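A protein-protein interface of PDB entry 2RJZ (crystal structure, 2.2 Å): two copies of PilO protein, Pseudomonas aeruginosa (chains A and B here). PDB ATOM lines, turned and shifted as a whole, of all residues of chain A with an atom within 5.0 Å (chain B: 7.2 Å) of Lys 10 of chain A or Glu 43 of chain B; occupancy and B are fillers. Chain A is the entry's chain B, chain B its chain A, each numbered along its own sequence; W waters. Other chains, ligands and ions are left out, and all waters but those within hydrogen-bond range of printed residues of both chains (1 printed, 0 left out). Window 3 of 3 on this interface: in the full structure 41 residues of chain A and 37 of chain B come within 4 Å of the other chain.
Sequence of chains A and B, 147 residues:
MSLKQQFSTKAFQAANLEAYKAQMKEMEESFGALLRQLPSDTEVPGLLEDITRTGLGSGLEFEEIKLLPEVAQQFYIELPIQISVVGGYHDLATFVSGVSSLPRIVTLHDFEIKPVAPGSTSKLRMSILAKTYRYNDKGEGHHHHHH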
ATOM      1  N   GLN A   6       7.755  10.677 -11.927  1.00  0.00           N
ATOM      2  CA  GLN A   6       9.050  11.344 -11.867  1.00  0.00           C
ATOM      3  C   GLN A   6       8.880  12.730 -11.251  1.00  0.00           C
ATOM      4  O   GLN A   6       9.671  13.144 -10.393  1.00  0.00           O
ATOM      5  CB  GLN A   6       9.723  11.401 -13.241  1.00  0.00           C
ATOM      6  CG  GLN A   6      10.310  10.026 -13.699  1.00  0.00           C
ATOM      7  CD  GLN A   6      10.749  10.007 -15.158  1.00  0.00           C
ATOM      8  OE1 GLN A   6      10.459  10.945 -15.926  1.00  0.00           O
ATOM      9  NE2 GLN A   6      11.484   8.967 -15.545  1.00  0.00           N
ATOM     10  N   PHE A   7       7.849  13.449 -11.667  1.00  0.00           N
ATOM     11  CA  PHE A   7       7.592  14.754 -11.074  1.00  0.00           C
ATOM     12  C   PHE A   7       7.230  14.681  -9.563  1.00  0.00           C
ATOM     13  O   PHE A   7       7.731  15.505  -8.774  1.00  0.00           O
ATOM     14  CB  PHE A   7       6.541  15.511 -11.876  1.00  0.00           C
ATOM     15  CG  PHE A   7       7.086  16.176 -13.109  1.00  0.00           C
ATOM     16  CD1 PHE A   7       8.047  17.200 -13.001  1.00  0.00           C
ATOM     17  CD2 PHE A   7       6.623  15.815 -14.386  1.00  0.00           C
ATOM     18  CE1 PHE A   7       8.564  17.825 -14.142  1.00  0.00           C
ATOM     19  CE2 PHE A   7       7.128  16.440 -15.533  1.00  0.00           C
ATOM     20  CZ  PHE A   7       8.103  17.442 -15.413  1.00  0.00           C
ATOM     21  N   SER A   8       6.418  13.691  -9.155  1.00  0.00           N
ATOM     22  CA  SER A   8       6.000  13.592  -7.735  1.00  0.00           C
ATOM     23  C   SER A   8       7.226  13.383  -6.896  1.00  0.00           C
ATOM     24  O   SER A   8       7.384  13.990  -5.841  1.00  0.00           O
ATOM     25  CB  SER A   8       5.072  12.405  -7.448  1.00  0.00           C
ATOM     26  OG  SER A   8       3.950  12.394  -8.301  1.00  0.00           O
ATOM     27  N   THR A   9       8.073  12.475  -7.375  1.00  0.00           N
ATOM     28  CA  THR A   9       9.291  12.080  -6.715  1.00  0.00           C
ATOM     29  C   THR A   9      10.212  13.283  -6.495  1.00  0.00           C
ATOM     30  O   THR A   9      10.896  13.388  -5.467  1.00  0.00           O
ATOM     31  CB  THR A   9       9.950  10.952  -7.572  1.00  0.00           C
ATOM     32  OG1 THR A   9       9.227   9.725  -7.371  1.00  0.00           O
ATOM     33  CG2 THR A   9      11.377  10.732  -7.221  1.00  0.00           C
ATOM     34  N   LYS A  10      10.246  14.193  -7.457  1.00  0.00           N
ATOM     35  CA  LYS A  10      11.146  15.333  -7.374  1.00  0.00           C
ATOM     36  C   LYS A  10      10.484  16.540  -6.693  1.00  0.00           C
ATOM     37  O   LYS A  10      11.056  17.629  -6.655  1.00  0.00           O
ATOM     38  CB  LYS A  10      11.653  15.705  -8.781  1.00  0.00           C
ATOM     39  CG  LYS A  10      12.524  14.622  -9.397  1.00  0.00           C
ATOM     40  CD  LYS A  10      13.038  15.002 -10.776  1.00  0.00           C
ATOM     41  CE  LYS A  10      14.237  15.946 -10.713  1.00  0.00           C
ATOM     42  NZ  LYS A  10      15.324  15.375  -9.855  1.00  0.00           N
ATOM     43  N   ALA A  11       9.275  16.347  -6.171  1.00  0.00           N
ATOM     44  CA  ALA A  11       8.505  17.457  -5.615  1.00  0.00           C
ATOM     45  C   ALA A  11       9.226  18.178  -4.479  1.00  0.00           C
ATOM     46  O   ALA A  11       9.096  19.375  -4.349  1.00  0.00           O
ATOM     47  CB  ALA A  11       7.099  17.008  -5.178  1.00  0.00           C
ATOM     48  N   PHE A  12      10.024  17.455  -3.699  1.00  0.00           N
ATOM     49  CA  PHE A  12      10.730  18.033  -2.539  1.00  0.00           C
ATOM     50  C   PHE A  12      11.693  19.135  -2.962  1.00  0.00           C
ATOM     51  O   PHE A  12      12.055  19.999  -2.157  1.00  0.00           O
ATOM     52  CB  PHE A  12      11.478  16.938  -1.747  1.00  0.00           C
ATOM     53  CG  PHE A  12      12.720  16.405  -2.451  1.00  0.00           C
ATOM     54  CD1 PHE A  12      13.992  16.792  -2.039  1.00  0.00           C
ATOM     55  CD2 PHE A  12      12.609  15.494  -3.506  1.00  0.00           C
ATOM     56  CE1 PHE A  12      15.143  16.303  -2.671  1.00  0.00           C
ATOM     57  CE2 PHE A  12      13.755  14.998  -4.158  1.00  0.00           C
ATOM     58  CZ  PHE A  12      15.028  15.406  -3.743  1.00  0.00           C
ATOM     59  N   GLN A  13      12.109  19.091  -4.226  1.00  0.00           N
ATOM     60  CA  GLN A  13      13.069  20.035  -4.801  1.00  0.00           C
ATOM     61  C   GLN A  13      12.439  21.354  -5.257  1.00  0.00           C
ATOM     62  O   GLN A  13      13.148  22.326  -5.470  1.00  0.00           O
ATOM     63  CB  GLN A  13      13.803  19.388  -5.981  1.00  0.00           C
ATOM     64  CG  GLN A  13      14.788  18.302  -5.586  1.00  0.00           C
ATOM     65  CD  GLN A  13      15.449  17.634  -6.774  1.00  0.00           C
ATOM     66  OE1 GLN A  13      14.807  16.941  -7.560  1.00  0.00           O
ATOM     67  NE2 GLN A  13      16.748  17.825  -6.897  1.00  0.00           N
ATOM     68  N   ALA A  14      11.120  21.381  -5.395  1.00  0.00           N
ATOM     69  CA  ALA A  14      10.417  22.561  -5.892  1.00  0.00           C
ATOM     70  C   ALA A  14      10.502  23.754  -4.932  1.00  0.00           C
ATOM     71  O   ALA A  14      10.179  23.638  -3.728  1.00  0.00           O
ATOM     72  CB  ALA A  14       8.974  22.233  -6.154  1.00  0.00           C
ATOM     73  N   TYR A  20       3.992  23.881  -7.516  1.00  0.00           N
ATOM     74  CA  TYR A  20       4.406  22.690  -8.250  1.00  0.00           C
ATOM     75  C   TYR A  20       3.260  21.675  -8.384  1.00  0.00           C
ATOM     76  O   TYR A  20       2.997  21.168  -9.482  1.00  0.00           O
ATOM     77  CB  TYR A  20       5.606  22.087  -7.538  1.00  0.00           C
ATOM     78  CG  TYR A  20       6.349  20.964  -8.242  1.00  0.00           C
ATOM     79  CD1 TYR A  20       7.429  21.230  -9.092  1.00  0.00           C
ATOM     80  CD2 TYR A  20       6.017  19.628  -7.992  1.00  0.00           C
ATOM     81  CE1 TYR A  20       8.156  20.177  -9.684  1.00  0.00           C
ATOM     82  CE2 TYR A  20       6.722  18.574  -8.577  1.00  0.00           C
ATOM     83  CZ  TYR A  20       7.786  18.853  -9.414  1.00  0.00           C
ATOM     84  OH  TYR A  20       8.459  17.804  -9.983  1.00  0.00           O
ATOM     85  N   GLN B  37      10.759  25.112 -11.822  1.00  0.00           N
ATOM     86  CA  GLN B  37      10.687  24.942 -10.362  1.00  0.00           C
ATOM     87  C   GLN B  37      11.762  23.985  -9.840  1.00  0.00           C
ATOM     88  O   GLN B  37      12.020  23.921  -8.643  1.00  0.00           O
ATOM     89  CB  GLN B  37       9.311  24.432  -9.939  1.00  0.00           C
ATOM     90  CG  GLN B  37       8.188  25.425 -10.155  1.00  0.00           C
ATOM     91  CD  GLN B  37       7.448  25.720  -8.880  1.00  0.00           C
ATOM     92  OE1 GLN B  37       8.047  25.879  -7.814  1.00  0.00           O
ATOM     93  NE2 GLN B  37       6.137  25.812  -8.975  1.00  0.00           N
ATOM     94  N   LEU B  38      12.373  23.248 -10.756  1.00  0.00           N
ATOM     95  CA  LEU B  38      13.418  22.296 -10.441  1.00  0.00           C
ATOM     96  C   LEU B  38      14.786  22.863 -10.858  1.00  0.00           C
ATOM     97  O   LEU B  38      14.846  23.859 -11.606  1.00  0.00           O
ATOM     98  CB  LEU B  38      13.133  20.961 -11.156  1.00  0.00           C
ATOM     99  CG  LEU B  38      11.872  20.186 -10.754  1.00  0.00           C
ATOM    100  CD1 LEU B  38      11.606  19.065 -11.739  1.00  0.00           C
ATOM    101  CD2 LEU B  38      11.935  19.648  -9.316  1.00  0.00           C
ATOM    102  N   PRO B  39      15.891  22.266 -10.364  1.00  0.00           N
ATOM    103  CA  PRO B  39      17.196  22.634 -10.946  1.00  0.00           C
ATOM    104  C   PRO B  39      17.524  21.773 -12.188  1.00  0.00           C
ATOM    105  O   PRO B  39      18.605  21.171 -12.279  1.00  0.00           O
ATOM    106  CB  PRO B  39      18.171  22.346  -9.801  1.00  0.00           C
ATOM    107  CG  PRO B  39      17.526  21.150  -9.059  1.00  0.00           C
ATOM    108  CD  PRO B  39      16.021  21.283  -9.257  1.00  0.00           C
ATOM    109  N   SER B  40      16.594  21.721 -13.140  1.00  0.00           N
ATOM    110  CA  SER B  40      16.717  20.808 -14.305  1.00  0.00           C
ATOM    111  C   SER B  40      17.828  21.194 -15.289  1.00  0.00           C
ATOM    112  O   SER B  40      18.323  20.334 -16.023  1.00  0.00           O
ATOM    113  CB  SER B  40      15.388  20.651 -15.037  1.00  0.00           C
ATOM    114  OG  SER B  40      15.055  21.868 -15.674  1.00  0.00           O
ATOM    115  N   ASP B  41      18.235  22.465 -15.292  1.00  0.00           N
ATOM    116  CA  ASP B  41      19.404  22.888 -16.103  1.00  0.00           C
ATOM    117  C   ASP B  41      20.754  22.454 -15.487  1.00  0.00           C
ATOM    118  O   ASP B  41      21.810  22.903 -15.908  1.00  0.00           O
ATOM    119  CB  ASP B  41      19.366  24.393 -16.410  1.00  0.00           C
ATOM    120  CG  ASP B  41      19.534  25.273 -15.165  1.00  0.00           C
ATOM    121  OD1 ASP B  41      19.448  24.777 -13.997  1.00  0.00           O
ATOM    122  OD2 ASP B  41      19.748  26.496 -15.374  1.00  0.00           O
ATOM    123  N   THR B  42      20.689  21.552 -14.512  1.00  0.00           N
ATOM    124  CA  THR B  42      21.848  21.042 -13.770  1.00  0.00           C
ATOM    125  C   THR B  42      21.788  19.521 -13.651  1.00  0.00           C
ATOM    126  O   THR B  42      22.675  18.889 -13.055  1.00  0.00           O
ATOM    127  CB  THR B  42      21.848  21.637 -12.335  1.00  0.00           C
ATOM    128  OG1 THR B  42      22.049  23.050 -12.418  1.00  0.00           O
ATOM    129  CG2 THR B  42      22.946  20.991 -11.436  1.00  0.00           C
ATOM    130  N   GLU B  43      20.741  18.938 -14.225  1.00  0.00           N
ATOM    131  CA  GLU B  43      20.413  17.531 -14.009  1.00  0.00           C
ATOM    132  C   GLU B  43      21.147  16.554 -14.916  1.00  0.00           C
ATOM    133  O   GLU B  43      21.212  15.382 -14.591  1.00  0.00           O
ATOM    134  CB  GLU B  43      18.906  17.306 -14.189  1.00  0.00           C
ATOM    135  CG  GLU B  43      18.018  18.037 -13.181  1.00  0.00           C
ATOM    136  CD  GLU B  43      17.929  17.344 -11.838  1.00  0.00           C
ATOM    137  OE1 GLU B  43      17.387  16.218 -11.769  1.00  0.00           O
ATOM    138  OE2 GLU B  43      18.392  17.938 -10.841  1.00  0.00           O
ATOM    139  N   VAL B  44      21.657  17.011 -16.058  1.00  0.00           N
ATOM    140  CA  VAL B  44      22.342  16.117 -17.004  1.00  0.00           C
ATOM    141  C   VAL B  44      23.485  15.282 -16.397  1.00  0.00           C
ATOM    142  O   VAL B  44      23.496  14.068 -16.582  1.00  0.00           O
ATOM    143  CB  VAL B  44      22.812  16.843 -18.305  1.00  0.00           C
ATOM    144  CG1 VAL B  44      23.657  15.913 -19.205  1.00  0.00           C
ATOM    145  CG2 VAL B  44      21.615  17.332 -19.079  1.00  0.00           C
ATOM    146  N   PRO B  45      24.429  15.921 -15.651  1.00  0.00           N
ATOM    147  CA  PRO B  45      25.531  15.127 -15.117  1.00  0.00           C
ATOM    148  C   PRO B  45      25.066  14.106 -14.076  1.00  0.00           C
ATOM    149  O   PRO B  45      25.609  12.990 -14.011  1.00  0.00           O
ATOM    150  CB  PRO B  45      26.440  16.193 -14.455  1.00  0.00           C
ATOM    151  CG  PRO B  45      26.046  17.480 -15.098  1.00  0.00           C
ATOM    152  CD  PRO B  45      24.569  17.342 -15.273  1.00  0.00           C
ATOM    153  N   GLY B  46      24.092  14.514 -13.258  1.00  0.00           N
ATOM    154  CA  GLY B  46      23.474  13.636 -12.284  1.00  0.00           C
ATOM    155  C   GLY B  46      22.702  12.525 -12.979  1.00  0.00           C
ATOM    156  O   GLY B  46      22.773  11.349 -12.573  1.00  0.00           O
ATOM    157  N   LEU B  47      21.984  12.878 -14.039  1.00  0.00           N
ATOM    158  CA  LEU B  47      21.302  11.854 -14.841  1.00  0.00           C
ATOM    159  C   LEU B  47      22.296  10.800 -15.368  1.00  0.00           C
ATOM    160  O   LEU B  47      22.103   9.590 -15.183  1.00  0.00           O
ATOM    161  CB  LEU B  47      20.481  12.474 -15.997  1.00  0.00           C
ATOM    162  CG  LEU B  47      19.747  11.473 -16.910  1.00  0.00           C
ATOM    163  CD1 LEU B  47      18.723  10.644 -16.149  1.00  0.00           C
ATOM    164  CD2 LEU B  47      19.056  12.241 -18.012  1.00  0.00           C
ATOM    165  N   LEU B  48      23.372  11.271 -15.995  1.00  0.00           N
ATOM    166  CA  LEU B  48      24.392  10.371 -16.525  1.00  0.00           C
ATOM    167  C   LEU B  48      24.992   9.488 -15.461  1.00  0.00           C
ATOM    168  O   LEU B  48      25.220   8.301 -15.688  1.00  0.00           O
ATOM    169  CB  LEU B  48      25.484  11.143 -17.282  1.00  0.00           C
ATOM    170  CG  LEU B  48      24.980  11.899 -18.530  1.00  0.00           C
ATOM    171  CD1 LEU B  48      26.173  12.477 -19.306  1.00  0.00           C
ATOM    172  CD2 LEU B  48      24.099  11.032 -19.460  1.00  0.00           C
ATOM    173  N   GLU B  49      25.218  10.061 -14.290  1.00  0.00           N
ATOM    174  CA  GLU B  49      25.694   9.284 -13.145  1.00  0.00           C
ATOM    175  C   GLU B  49      24.703   8.158 -12.761  1.00  0.00           C
ATOM    176  O   GLU B  49      25.116   7.039 -12.504  1.00  0.00           O
ATOM    177  CB  GLU B  49      25.915  10.210 -11.944  1.00  0.00           C
ATOM    178  CG  GLU B  49      26.271   9.456 -10.689  1.00  0.00           C
ATOM    179  CD  GLU B  49      25.999  10.239  -9.437  1.00  0.00           C
ATOM    180  OE1 GLU B  49      25.115  11.135  -9.459  1.00  0.00           O
ATOM    181  OE2 GLU B  49      26.658   9.946  -8.416  1.00  0.00           O
ATOM    182  N   ASP B  50      23.407   8.471 -12.689  1.00  0.00           N
ATOM    183  CA  ASP B  50      22.389   7.464 -12.318  1.00  0.00           C
ATOM    184  C   ASP B  50      22.205   6.415 -13.387  1.00  0.00           C
ATOM    185  O   ASP B  50      22.087   5.232 -13.082  1.00  0.00           O
ATOM    186  CB  ASP B  50      21.034   8.120 -12.061  1.00  0.00           C
ATOM    187  CG  ASP B  50      20.991   8.850 -10.749  1.00  0.00           C
ATOM    188  OD1 ASP B  50      21.820   8.508  -9.887  1.00  0.00           O
ATOM    189  OD2 ASP B  50      20.132   9.757 -10.574  1.00  0.00           O
ATOM    190  N   LEU B 102      13.883   6.087 -12.225  1.00  0.00           N
ATOM    191  CA  LEU B 102      14.784   7.038 -11.563  1.00  0.00           C
ATOM    192  C   LEU B 102      14.079   8.322 -11.115  1.00  0.00           C
ATOM    193  O   LEU B 102      13.112   8.762 -11.758  1.00  0.00           O
ATOM    194  CB  LEU B 102      15.922   7.450 -12.502  1.00  0.00           C
ATOM    195  CG  LEU B 102      17.028   6.463 -12.883  1.00  0.00           C
ATOM    196  CD1 LEU B 102      17.951   7.084 -13.968  1.00  0.00           C
ATOM    197  CD2 LEU B 102      17.822   6.049 -11.661  1.00  0.00           C
ATOM    198  N   PRO B 103      14.590   8.967 -10.043  1.00  0.00           N
ATOM    199  CA  PRO B 103      13.993  10.222  -9.596  1.00  0.00           C
ATOM    200  C   PRO B 103      14.503  11.381 -10.451  1.00  0.00           C
ATOM    201  O   PRO B 103      15.105  12.325  -9.920  1.00  0.00           O
ATOM    202  CB  PRO B 103      14.507  10.372  -8.147  1.00  0.00           C
ATOM    203  CG  PRO B 103      15.441   9.204  -7.903  1.00  0.00           C
ATOM    204  CD  PRO B 103      15.757   8.601  -9.218  1.00  0.00           C
ATOM    205  N   ARG B 104      14.299  11.270 -11.766  1.00  0.00           N
ATOM    206  CA  ARG B 104      14.763  12.246 -12.758  1.00  0.00           C
ATOM    207  C   ARG B 104      13.666  12.356 -13.815  1.00  0.00           C
ATOM    208  O   ARG B 104      12.877  11.414 -13.994  1.00  0.00           O
ATOM    209  CB  ARG B 104      16.052  11.762 -13.456  1.00  0.00           C
ATOM    210  CG  ARG B 104      17.241  11.443 -12.531  1.00  0.00           C
ATOM    211  CD  ARG B 104      18.183  12.634 -12.398  1.00  0.00           C
ATOM    212  NE  ARG B 104      19.228  12.347 -11.423  1.00  0.00           N
ATOM    213  CZ  ARG B 104      19.940  13.281 -10.798  1.00  0.00           C
ATOM    214  NH1 ARG B 104      19.711  14.560 -11.059  1.00  0.00           N
ATOM    215  NH2 ARG B 104      20.883  12.932  -9.922  1.00  0.00           N
ATOM    216  N   ILE B 105      13.643  13.481 -14.523  1.00  0.00           N
ATOM    217  CA  ILE B 105      12.732  13.706 -15.628  1.00  0.00           C
ATOM    218  C   ILE B 105      13.463  13.156 -16.862  1.00  0.00           C
ATOM    219  O   ILE B 105      14.280  13.838 -17.480  1.00  0.00           O
ATOM    220  CB  ILE B 105      12.378  15.231 -15.832  1.00  0.00           C
ATOM    221  CG1 ILE B 105      11.930  15.921 -14.523  1.00  0.00           C
ATOM    222  CG2 ILE B 105      11.399  15.403 -17.004  1.00  0.00           C
ATOM    223  CD1 ILE B 105      10.825  15.234 -13.744  1.00  0.00           C
ATOM    224  N   VAL B 106      13.203  11.889 -17.162  1.00  0.00           N
ATOM    225  CA  VAL B 106      13.880  11.203 -18.257  1.00  0.00           C
ATOM    226  C   VAL B 106      12.878  10.271 -18.946  1.00  0.00           C
ATOM    227  O   VAL B 106      12.180   9.516 -18.281  1.00  0.00           O
ATOM    228  CB  VAL B 106      15.162  10.449 -17.785  1.00  0.00           C
ATOM    229  CG1 VAL B 106      14.841   9.415 -16.709  1.00  0.00           C
ATOM    230  CG2 VAL B 106      15.892   9.815 -18.970  1.00  0.00           C
ATOM    231  N   THR B 132      16.155  14.046 -21.829  1.00  0.00           N
ATOM    232  CA  THR B 132      15.819  14.845 -20.699  1.00  0.00           C
ATOM    233  C   THR B 132      15.471  16.250 -21.212  1.00  0.00           C
ATOM    234  O   THR B 132      15.607  16.543 -22.411  1.00  0.00           O
ATOM    235  CB  THR B 132      16.923  14.808 -19.620  1.00  0.00           C
ATOM    236  OG1 THR B 132      16.364  15.291 -18.379  1.00  0.00           O
ATOM    237  CG2 THR B 132      18.159  15.634 -20.053  1.00  0.00           C
ATOM    238  N   TYR B 133      15.034  17.104 -20.299  1.00  0.00           N
ATOM    239  CA  TYR B 133      14.399  18.344 -20.649  1.00  0.00           C
ATOM    240  C   TYR B 133      14.787  19.449 -19.655  1.00  0.00           C
ATOM    241  O   TYR B 133      15.018  19.202 -18.458  1.00  0.00           O
ATOM    242  CB  TYR B 133      12.863  18.174 -20.668  1.00  0.00           C
ATOM    243  CG  TYR B 133      12.362  16.963 -21.462  1.00  0.00           C
ATOM    244  CD1 TYR B 133      11.878  17.096 -22.783  1.00  0.00           C
ATOM    245  CD2 TYR B 133      12.385  15.687 -20.888  1.00  0.00           C
ATOM    246  CE1 TYR B 133      11.413  15.963 -23.489  1.00  0.00           C
ATOM    247  CE2 TYR B 133      11.952  14.575 -21.570  1.00  0.00           C
ATOM    248  CZ  TYR B 133      11.465  14.706 -22.860  1.00  0.00           C
ATOM    249  OH  TYR B 133      11.051  13.545 -23.479  1.00  0.00           O
HETATM  250  O   HOH W   1       9.047   9.314 -17.779  1.00  0.00           O
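NE2 of Gln 37 of chain B sits close to N of Tyr 20 of chain A (3.2 Å). The side-chain carboxylate of Glu 43 of chain B lies within salt-bridge range of the side-chain amino group of Lys 10 of chain A (2.9 Å). O of Pro 103 of chain B is in hydrogen-bond range of NZ of Lys 10 of chain A (3.1 Å). O of Arg 104 of chain B lies close to OE1 of Gln 6 of chain A. The backbone carbonyl oxygen of Val 106 of chain B is in hydrogen-bond range of the side-chain amide nitrogen of Gln 6 of chain A, 2.9 Å away.
No position is printed for both chains. Of the 16 pairs that touch across the chains among the printed residues, none has its exchanged pair printed and touching as well.
Of the printed residues of chain B, Thr 9 of chain A touches Pro 103. Lys 10 of chain A touches five residues of chain B. Glu 43 of chain B touches just one residue of chain A: Lys 10. Of the printed residues of chain A, Arg 104 of chain B touches Gln 6 (2.8 Å) and Lys 10 (3.8 Å). The nearest residue of chain B that does not touch Lys 10 of chain A is Pro 39 of chain B (5.8 Å). The nearest residue of chain A that does not touch Glu 43 of chain B is Gln 13 of chain A (4.3 Å). The nearest printed residue of chain A that does not touch Ile 105 of chain B is Tyr 20 of chain A (5.1 Å).
OE1 of Glu 43 of chain B lies within salt-bridge range of NH1 of Arg 104 of chain B (2.9 Å). The side-chain carboxylate (OD2) of Asp 50 of chain B is in salt-bridge range of the guanidinium group (NE) of Arg 104 of chain B (2.9 Å). The backbone carbonyl oxygen (O) of Ile 105 of chain B sits at hydrogen-bond distance from the side-chain hydroxyl (OG1) of Thr 132 of chain B (2.7 Å). The backbone carbonyl oxygen of Phe 7 of chain A lies within hydrogen-bond range of the side-chain hydroxyl of Tyr 20 of chain A, at 2.7 Å. The side-chain amino group (NZ) of Lys 10 of chain A sits at hydrogen-bond distance from the side-chain amide oxygen (OE1) of Gln 13 of chain A, at 2.8 Å.
Water W1 bridges the side-chain amide oxygen (OE1) of Gln 6 of chain A and the backbone carbonyl oxygen (O) of Val 106 of chain B.
Leu 102 of chain B touches Gln 6 of chain A. Ile 105 of chain B touches Gln 6 of chain A (CA to OE1, 3.6 Å). Phe 7 of chain A touches Ile 105 of chain B (CE1 to CD1, 3.5 Å). Pro 103 of chain B touches Thr 9 of chain A (CB to CG2, 3.3 Å). Lys 10 of chain A touches Leu 38 of chain B. Arg 104 of chain B touches Lys 10 of chain A. Lys 10 of chain A touches Ile 105 of chain B. Gln 37 of chain B touches Gln 13 of chain A (O to O, 3.7 Å). CA of Ala 14 of chain A touches O of Gln 37 of chain B, 3.5 Å away. OH of Tyr 20 of chain A touches CD1 of Leu 38 of chain B, 3.8 Å away.
Along chain B the printed residues that touch a printed residue of chain A span positions 37 to 106. Hydrophobic or aromatic side chains of chain A within 4 Å of the printed part of chain B: Phe 7 and Tyr 20. Along chain A the printed residues that touch a printed residue of chain B span positions 6 to 20. Among the printed residues, 16 pairs touch across the chains.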
